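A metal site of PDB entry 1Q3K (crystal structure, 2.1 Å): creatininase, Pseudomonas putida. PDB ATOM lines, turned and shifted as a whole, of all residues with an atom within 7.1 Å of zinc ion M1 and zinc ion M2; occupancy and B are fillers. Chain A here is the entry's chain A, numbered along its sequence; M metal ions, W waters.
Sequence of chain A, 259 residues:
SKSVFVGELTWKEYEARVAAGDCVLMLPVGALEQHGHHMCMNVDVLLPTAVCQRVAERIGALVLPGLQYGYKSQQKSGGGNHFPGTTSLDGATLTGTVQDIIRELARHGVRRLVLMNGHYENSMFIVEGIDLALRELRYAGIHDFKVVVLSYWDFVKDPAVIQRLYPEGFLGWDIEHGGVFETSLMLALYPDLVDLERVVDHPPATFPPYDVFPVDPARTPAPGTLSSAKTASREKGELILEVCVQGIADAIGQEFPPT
Zinc ion M2 is bound by OE2 of Glu 182, water W1, OD1 of Asp 44 and NE2 of His 35. Zinc ion M2 has four donor atoms within binding distance. Slightly farther from zinc ion M2 lies OE1 of Glu 182 (2.8 Å).
The side-chain carboxylate (OE1) of Glu 182 lies within hydrogen-bond range of the backbone NH (N) of Gly 178 (2.7 Å). The backbone carbonyl oxygen of Glu 33 is in hydrogen-bond range of a ring nitrogen (ND1) of His 35, at 2.7 Å. The side-chain carboxylate (OE2) of Glu 33 lies within hydrogen-bond range of the side-chain hydroxyl (OG) of Ser 73 (2.6 Å). NE2 of His 119 sits close to OE1 of Glu 121 (3.4 Å). The backbone carbonyl oxygen (O) of Tyr 71 is in hydrogen-bond range of a ring nitrogen (NE2) of His 119 (2.9 Å). O of Gly 78 sits at hydrogen-bond distance from NE2 of His 177 (3.0 Å). A ring nitrogen (NE2) of His 177 lies within hydrogen-bond range of the backbone carbonyl oxygen of Gln 34, at 2.9 Å.
Water W1 bridges a ring nitrogen (ND1) of His 177 (2.5 Å) and the side-chain carboxylate of Glu 182 (3.5 Å).
His 177 touches zinc ion M2. Of the 24 residues printed, 4 come within 4 Å of zinc ion M2. Along chain A the residues within 4 Å of zinc ion M2 span positions 35 to 182. The nearest printed residue that does not touch zinc ion M2 is Val 43 (4.2 Å).
Of the 24 residues printed, 3 come within 4 Å of zinc ion M1. The nearest printed residue that does not touch zinc ion M1 is His 177 (4.04 Å).
OD2 of Asp 44 binds zinc ion M1. OE1 of Glu 33 is bound to zinc ion M1. Zinc ion M1 is bound by ND1 of His 119, 2.4 Å away. Water W2 binds zinc ion M1 (2.4 Å). Water W1 binds zinc ion M1 (2.5 Å). Zinc ion M1 is bound by water W3, 2.7 Å away.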
ATOM      1  N   GLY A  30      -7.122   6.856  15.369  1.00  0.00           N
ATOM      2  CA  GLY A  30      -7.235   8.234  14.890  1.00  0.00           C
ATOM      3  C   GLY A  30      -6.036   8.746  14.080  1.00  0.00           C
ATOM      4  O   GLY A  30      -5.528   8.046  13.231  1.00  0.00           O
ATOM      5  N   ALA A  31      -5.598   9.967  14.380  1.00  0.00           N
ATOM      6  CA  ALA A  31      -4.515  10.634  13.674  1.00  0.00           C
ATOM      7  C   ALA A  31      -4.120  11.913  14.391  1.00  0.00           C
ATOM      8  O   ALA A  31      -4.810  12.345  15.318  1.00  0.00           O
ATOM      9  CB  ALA A  31      -4.937  10.945  12.285  1.00  0.00           C
ATOM     10  N   GLU A  33      -3.510  15.332  13.034  1.00  0.00           N
ATOM     11  CA  GLU A  33      -3.739  16.079  11.837  1.00  0.00           C
ATOM     12  C   GLU A  33      -4.319  17.508  12.044  1.00  0.00           C
ATOM     13  O   GLU A  33      -5.161  17.759  12.884  1.00  0.00           O
ATOM     14  CB  GLU A  33      -4.708  15.237  10.979  1.00  0.00           C
ATOM     15  CG  GLU A  33      -5.166  15.797   9.660  1.00  0.00           C
ATOM     16  CD  GLU A  33      -6.274  14.971   9.077  1.00  0.00           C
ATOM     17  OE1 GLU A  33      -7.183  14.556   9.837  1.00  0.00           O
ATOM     18  OE2 GLU A  33      -6.301  14.710   7.843  1.00  0.00           O
ATOM     19  N   GLN A  34      -3.819  18.460  11.274  1.00  0.00           N
ATOM     20  CA  GLN A  34      -4.296  19.822  11.325  1.00  0.00           C
ATOM     21  C   GLN A  34      -5.826  19.817  11.149  1.00  0.00           C
ATOM     22  O   GLN A  34      -6.393  19.021  10.383  1.00  0.00           O
ATOM     23  CB  GLN A  34      -3.649  20.656  10.229  1.00  0.00           C
ATOM     24  CG  GLN A  34      -3.993  20.257   8.827  1.00  0.00           C
ATOM     25  CD  GLN A  34      -5.347  20.732   8.356  1.00  0.00           C
ATOM     26  OE1 GLN A  34      -5.919  20.171   7.369  1.00  0.00           O
ATOM     27  NE2 GLN A  34      -5.883  21.750   8.988  1.00  0.00           N
ATOM     28  N   HIS A  35      -6.493  20.662  11.907  1.00  0.00           N
ATOM     29  CA  HIS A  35      -7.922  20.786  11.847  1.00  0.00           C
ATOM     30  C   HIS A  35      -8.264  22.282  11.834  1.00  0.00           C
ATOM     31  O   HIS A  35      -9.003  22.765  12.679  1.00  0.00           O
ATOM     32  CB  HIS A  35      -8.585  20.079  13.041  1.00  0.00           C
ATOM     33  CG  HIS A  35      -8.869  18.622  12.777  1.00  0.00           C
ATOM     34  ND1 HIS A  35      -7.875  17.666  12.781  1.00  0.00           N
ATOM     35  CD2 HIS A  35     -10.008  17.987  12.454  1.00  0.00           C
ATOM     36  CE1 HIS A  35      -8.405  16.491  12.521  1.00  0.00           C
ATOM     37  NE2 HIS A  35      -9.701  16.658  12.314  1.00  0.00           N
ATOM     38  N   MET A  39      -9.318  24.459  15.910  1.00  0.00           N
ATOM     39  CA  MET A  39      -9.262  23.249  16.764  1.00  0.00           C
ATOM     40  C   MET A  39      -7.852  22.666  16.852  1.00  0.00           C
ATOM     41  O   MET A  39      -7.003  22.893  16.005  1.00  0.00           O
ATOM     42  CB  MET A  39     -10.155  22.134  16.236  1.00  0.00           C
ATOM     43  CG  MET A  39     -11.603  22.315  16.481  1.00  0.00           C
ATOM     44  SD  MET A  39     -12.507  20.807  16.126  1.00  0.00           S
ATOM     45  CE  MET A  39     -12.337  20.700  14.371  1.00  0.00           C
ATOM     46  N   VAL A  43      -7.950  15.714  17.403  1.00  0.00           N
ATOM     47  CA  VAL A  43      -9.388  15.516  17.264  1.00  0.00           C
ATOM     48  C   VAL A  43      -9.746  14.078  16.890  1.00  0.00           C
ATOM     49  O   VAL A  43     -10.536  13.432  17.566  1.00  0.00           O
ATOM     50  CB  VAL A  43      -9.923  16.462  16.204  1.00  0.00           C
ATOM     51  CG1 VAL A  43     -11.350  16.154  15.854  1.00  0.00           C
ATOM     52  CG2 VAL A  43      -9.803  17.907  16.656  1.00  0.00           C
ATOM     53  N   ASP A  44      -9.131  13.584  15.807  1.00  0.00           N
ATOM     54  CA  ASP A  44      -9.412  12.221  15.287  1.00  0.00           C
ATOM     55  C   ASP A  44      -9.129  11.128  16.306  1.00  0.00           C
ATOM     56  O   ASP A  44      -9.649  10.019  16.192  1.00  0.00           O
ATOM     57  CB  ASP A  44      -8.685  11.950  13.972  1.00  0.00           C
ATOM     58  CG  ASP A  44      -9.229  12.774  12.825  1.00  0.00           C
ATOM     59  OD1 ASP A  44     -10.150  13.540  13.153  1.00  0.00           O
ATOM     60  OD2 ASP A  44      -8.805  12.741  11.616  1.00  0.00           O
ATOM     61  N   VAL A  45      -8.360  11.424  17.333  1.00  0.00           N
ATOM     62  CA  VAL A  45      -8.109  10.432  18.364  1.00  0.00           C
ATOM     63  C   VAL A  45      -9.077  10.687  19.552  1.00  0.00           C
ATOM     64  O   VAL A  45      -9.681   9.738  20.125  1.00  0.00           O
ATOM     65  CB  VAL A  45      -6.668  10.517  18.873  1.00  0.00           C
ATOM     66  CG1 VAL A  45      -6.469   9.525  19.946  1.00  0.00           C
ATOM     67  CG2 VAL A  45      -5.673  10.240  17.759  1.00  0.00           C
ATOM     68  N   LEU A  47     -12.094  12.221  19.627  1.00  0.00           N
ATOM     69  CA  LEU A  47     -13.470  11.947  19.332  1.00  0.00           C
ATOM     70  C   LEU A  47     -13.789  10.454  19.412  1.00  0.00           C
ATOM     71  O   LEU A  47     -14.664  10.083  20.182  1.00  0.00           O
ATOM     72  CB  LEU A  47     -13.891  12.494  17.960  1.00  0.00           C
ATOM     73  CG  LEU A  47     -13.791  14.023  17.971  1.00  0.00           C
ATOM     74  CD1 LEU A  47     -14.346  14.634  16.700  1.00  0.00           C
ATOM     75  CD2 LEU A  47     -14.574  14.575  19.170  1.00  0.00           C
ATOM     76  N   TYR A  71      -2.957   7.208   8.872  1.00  0.00           N
ATOM     77  CA  TYR A  71      -2.485   7.292   7.524  1.00  0.00           C
ATOM     78  C   TYR A  71      -2.426   8.756   7.054  1.00  0.00           C
ATOM     79  O   TYR A  71      -3.082   9.668   7.569  1.00  0.00           O
ATOM     80  CB  TYR A  71      -3.296   6.434   6.568  1.00  0.00           C
ATOM     81  CG  TYR A  71      -2.665   6.416   5.178  1.00  0.00           C
ATOM     82  CD1 TYR A  71      -1.417   5.863   4.976  1.00  0.00           C
ATOM     83  CD2 TYR A  71      -3.280   7.026   4.098  1.00  0.00           C
ATOM     84  CE1 TYR A  71      -0.827   5.875   3.777  1.00  0.00           C
ATOM     85  CE2 TYR A  71      -2.681   6.996   2.881  1.00  0.00           C
ATOM     86  CZ  TYR A  71      -1.421   6.468   2.735  1.00  0.00           C
ATOM     87  OH  TYR A  71      -0.765   6.454   1.536  1.00  0.00           O
ATOM     88  N   SER A  73      -2.800  12.143   5.426  1.00  0.00           N
ATOM     89  CA  SER A  73      -3.973  12.945   5.147  1.00  0.00           C
ATOM     90  C   SER A  73      -4.057  13.137   3.627  1.00  0.00           C
ATOM     91  O   SER A  73      -3.088  13.436   2.965  1.00  0.00           O
ATOM     92  CB  SER A  73      -3.818  14.346   5.888  1.00  0.00           C
ATOM     93  OG  SER A  73      -4.978  15.112   5.672  1.00  0.00           O
ATOM     94  N   SER A  77     -10.136  14.730   1.779  1.00  0.00           N
ATOM     95  CA  SER A  77     -10.857  14.314   2.958  1.00  0.00           C
ATOM     96  C   SER A  77     -10.260  14.867   4.215  1.00  0.00           C
ATOM     97  O   SER A  77     -10.922  14.848   5.243  1.00  0.00           O
ATOM     98  CB  SER A  77     -10.933  12.790   3.038  1.00  0.00           C
ATOM     99  OG  SER A  77      -9.612  12.248   3.101  1.00  0.00           O
ATOM    100  N   GLY A  78      -9.024  15.303   4.180  1.00  0.00           N
ATOM    101  CA  GLY A  78      -8.358  15.826   5.372  1.00  0.00           C
ATOM    102  C   GLY A  78      -7.475  17.035   5.124  1.00  0.00           C
ATOM    103  O   GLY A  78      -6.832  17.522   6.014  1.00  0.00           O
ATOM    104  N   GLY A 118     -11.491   7.145  13.654  1.00  0.00           N
ATOM    105  CA  GLY A 118     -11.833   8.546  13.717  1.00  0.00           C
ATOM    106  C   GLY A 118     -11.216   9.347  12.562  1.00  0.00           C
ATOM    107  O   GLY A 118     -11.507  10.535  12.365  1.00  0.00           O
ATOM    108  N   HIS A 119     -10.361   8.702  11.783  1.00  0.00           N
ATOM    109  CA  HIS A 119      -9.646   9.350  10.663  1.00  0.00           C
ATOM    110  C   HIS A 119      -9.974   8.635   9.318  1.00  0.00           C
ATOM    111  O   HIS A 119      -9.608   7.470   9.104  1.00  0.00           O
ATOM    112  CB  HIS A 119      -8.150   9.389  10.989  1.00  0.00           C
ATOM    113  CG  HIS A 119      -7.275   9.962   9.930  1.00  0.00           C
ATOM    114  ND1 HIS A 119      -7.388  11.248   9.471  1.00  0.00           N
ATOM    115  CD2 HIS A 119      -6.214   9.427   9.268  1.00  0.00           C
ATOM    116  CE1 HIS A 119      -6.472  11.481   8.556  1.00  0.00           C
ATOM    117  NE2 HIS A 119      -5.767  10.376   8.389  1.00  0.00           N
ATOM    118  N   TYR A 120     -10.750   9.306   8.478  1.00  0.00           N
ATOM    119  CA  TYR A 120     -11.246   8.795   7.184  1.00  0.00           C
ATOM    120  C   TYR A 120     -10.219   7.938   6.404  1.00  0.00           C
ATOM    121  O   TYR A 120     -10.503   6.862   5.928  1.00  0.00           O
ATOM    122  CB  TYR A 120     -11.617  10.000   6.321  1.00  0.00           C
ATOM    123  CG  TYR A 120     -12.508   9.720   5.161  1.00  0.00           C
ATOM    124  CD1 TYR A 120     -13.903   9.765   5.307  1.00  0.00           C
ATOM    125  CD2 TYR A 120     -11.982   9.487   3.904  1.00  0.00           C
ATOM    126  CE1 TYR A 120     -14.739   9.528   4.225  1.00  0.00           C
ATOM    127  CE2 TYR A 120     -12.794   9.221   2.815  1.00  0.00           C
ATOM    128  CZ  TYR A 120     -14.187   9.252   2.975  1.00  0.00           C
ATOM    129  OH  TYR A 120     -15.030   8.981   1.888  1.00  0.00           O
ATOM    130  N   GLU A 121      -9.014   8.472   6.273  1.00  0.00           N
ATOM    131  CA  GLU A 121      -7.977   7.823   5.523  1.00  0.00           C
ATOM    132  C   GLU A 121      -7.440   6.492   6.090  1.00  0.00           C
ATOM    133  O   GLU A 121      -6.784   5.786   5.380  1.00  0.00           O
ATOM    134  CB  GLU A 121      -6.836   8.791   5.342  1.00  0.00           C
ATOM    135  CG  GLU A 121      -7.204   9.959   4.483  1.00  0.00           C
ATOM    136  CD  GLU A 121      -7.674  11.189   5.241  1.00  0.00           C
ATOM    137  OE1 GLU A 121      -8.366  11.028   6.258  1.00  0.00           O
ATOM    138  OE2 GLU A 121      -7.368  12.302   4.781  1.00  0.00           O
ATOM    139  N   TYR A 152     -17.240   6.104  13.413  1.00  0.00           N
ATOM    140  CA  TYR A 152     -18.324   6.569  14.273  1.00  0.00           C
ATOM    141  C   TYR A 152     -19.307   7.503  13.556  1.00  0.00           C
ATOM    142  O   TYR A 152     -20.480   7.391  13.779  1.00  0.00           O
ATOM    143  CB  TYR A 152     -17.801   7.188  15.603  1.00  0.00           C
ATOM    144  CG  TYR A 152     -17.160   8.548  15.440  1.00  0.00           C
ATOM    145  CD1 TYR A 152     -17.936   9.731  15.424  1.00  0.00           C
ATOM    146  CD2 TYR A 152     -15.783   8.679  15.309  1.00  0.00           C
ATOM    147  CE1 TYR A 152     -17.329  10.962  15.248  1.00  0.00           C
ATOM    148  CE2 TYR A 152     -15.186   9.921  15.162  1.00  0.00           C
ATOM    149  CZ  TYR A 152     -15.947  11.049  15.128  1.00  0.00           C
ATOM    150  OH  TYR A 152     -15.351  12.253  14.955  1.00  0.00           O
ATOM    151  N   TRP A 153     -18.855   8.372  12.647  1.00  0.00           N
ATOM    152  CA  TRP A 153     -19.781   9.273  11.987  1.00  0.00           C
ATOM    153  C   TRP A 153     -20.808   8.555  11.068  1.00  0.00           C
ATOM    154  O   TRP A 153     -21.869   9.083  10.721  1.00  0.00           O
ATOM    155  CB  TRP A 153     -19.040  10.348  11.190  1.00  0.00           C
ATOM    156  CG  TRP A 153     -18.132   9.810  10.157  1.00  0.00           C
ATOM    157  CD1 TRP A 153     -18.487   9.332   8.912  1.00  0.00           C
ATOM    158  CD2 TRP A 153     -16.697   9.658  10.244  1.00  0.00           C
ATOM    159  NE1 TRP A 153     -17.366   8.898   8.241  1.00  0.00           N
ATOM    160  CE2 TRP A 153     -16.262   9.072   9.043  1.00  0.00           C
ATOM    161  CE3 TRP A 153     -15.754   9.950  11.227  1.00  0.00           C
ATOM    162  CZ2 TRP A 153     -14.910   8.807   8.788  1.00  0.00           C
ATOM    163  CZ3 TRP A 153     -14.390   9.652  10.978  1.00  0.00           C
ATOM    164  CH2 TRP A 153     -13.998   9.094   9.773  1.00  0.00           C
ATOM    165  N   GLU A 176     -16.236  16.926   5.572  1.00  0.00           N
ATOM    166  CA  GLU A 176     -16.455  17.141   6.978  1.00  0.00           C
ATOM    167  C   GLU A 176     -15.159  17.141   7.772  1.00  0.00           C
ATOM    168  O   GLU A 176     -15.063  16.475   8.819  1.00  0.00           O
ATOM    169  CB  GLU A 176     -17.393  16.095   7.552  1.00  0.00           C
ATOM    170  CG  GLU A 176     -18.872  16.473   7.510  1.00  0.00           C
ATOM    171  CD  GLU A 176     -19.181  17.810   8.184  1.00  0.00           C
ATOM    172  OE1 GLU A 176     -18.616  18.159   9.241  1.00  0.00           O
ATOM    173  OE2 GLU A 176     -20.035  18.545   7.654  1.00  0.00           O
ATOM    174  N   HIS A 177     -14.127  17.811   7.260  1.00  0.00           N
ATOM    175  CA  HIS A 177     -12.865  17.831   7.964  1.00  0.00           C
ATOM    176  C   HIS A 177     -12.685  19.186   8.617  1.00  0.00           C
ATOM    177  O   HIS A 177     -12.396  20.169   7.961  1.00  0.00           O
ATOM    178  CB  HIS A 177     -11.685  17.577   7.026  1.00  0.00           C
ATOM    179  CG  HIS A 177     -10.361  17.792   7.688  1.00  0.00           C
ATOM    180  ND1 HIS A 177      -9.874  16.974   8.675  1.00  0.00           N
ATOM    181  CD2 HIS A 177      -9.413  18.736   7.480  1.00  0.00           C
ATOM    182  CE1 HIS A 177      -8.681  17.392   9.049  1.00  0.00           C
ATOM    183  NE2 HIS A 177      -8.386  18.464   8.352  1.00  0.00           N
ATOM    184  N   GLY A 178     -12.791  19.191   9.933  1.00  0.00           N
ATOM    185  CA  GLY A 178     -12.692  20.416  10.704  1.00  0.00           C
ATOM    186  C   GLY A 178     -13.971  21.236  10.590  1.00  0.00           C
ATOM    187  O   GLY A 178     -14.012  22.373  10.984  1.00  0.00           O
ATOM    188  N   GLU A 182     -17.380  17.646  13.377  1.00  0.00           N
ATOM    189  CA  GLU A 182     -16.296  17.507  14.352  1.00  0.00           C
ATOM    190  C   GLU A 182     -16.245  18.656  15.396  1.00  0.00           C
ATOM    191  O   GLU A 182     -16.129  18.412  16.598  1.00  0.00           O
ATOM    192  CB  GLU A 182     -14.933  17.409  13.662  1.00  0.00           C
ATOM    193  CG  GLU A 182     -14.722  16.152  12.830  1.00  0.00           C
ATOM    194  CD  GLU A 182     -13.300  16.035  12.270  1.00  0.00           C
ATOM    195  OE1 GLU A 182     -12.879  16.939  11.497  1.00  0.00           O
ATOM    196  OE2 GLU A 182     -12.621  15.015  12.605  1.00  0.00           O
HETATM  197 ZN    ZN M   1      -8.713  13.249   9.740  1.00  0.00          ZN
HETATM  198 ZN    ZN M   2     -10.893  14.952  11.884  1.00  0.00          ZN
HETATM  199  O   HOH W   1     -10.450  14.952  10.033  1.00  0.00           O
HETATM  200  O   HOH W   2      -8.555  13.423   7.335  1.00  0.00           O
HETATM  201  O   HOH W   3     -11.217  12.462   9.266  1.00  0.00           O
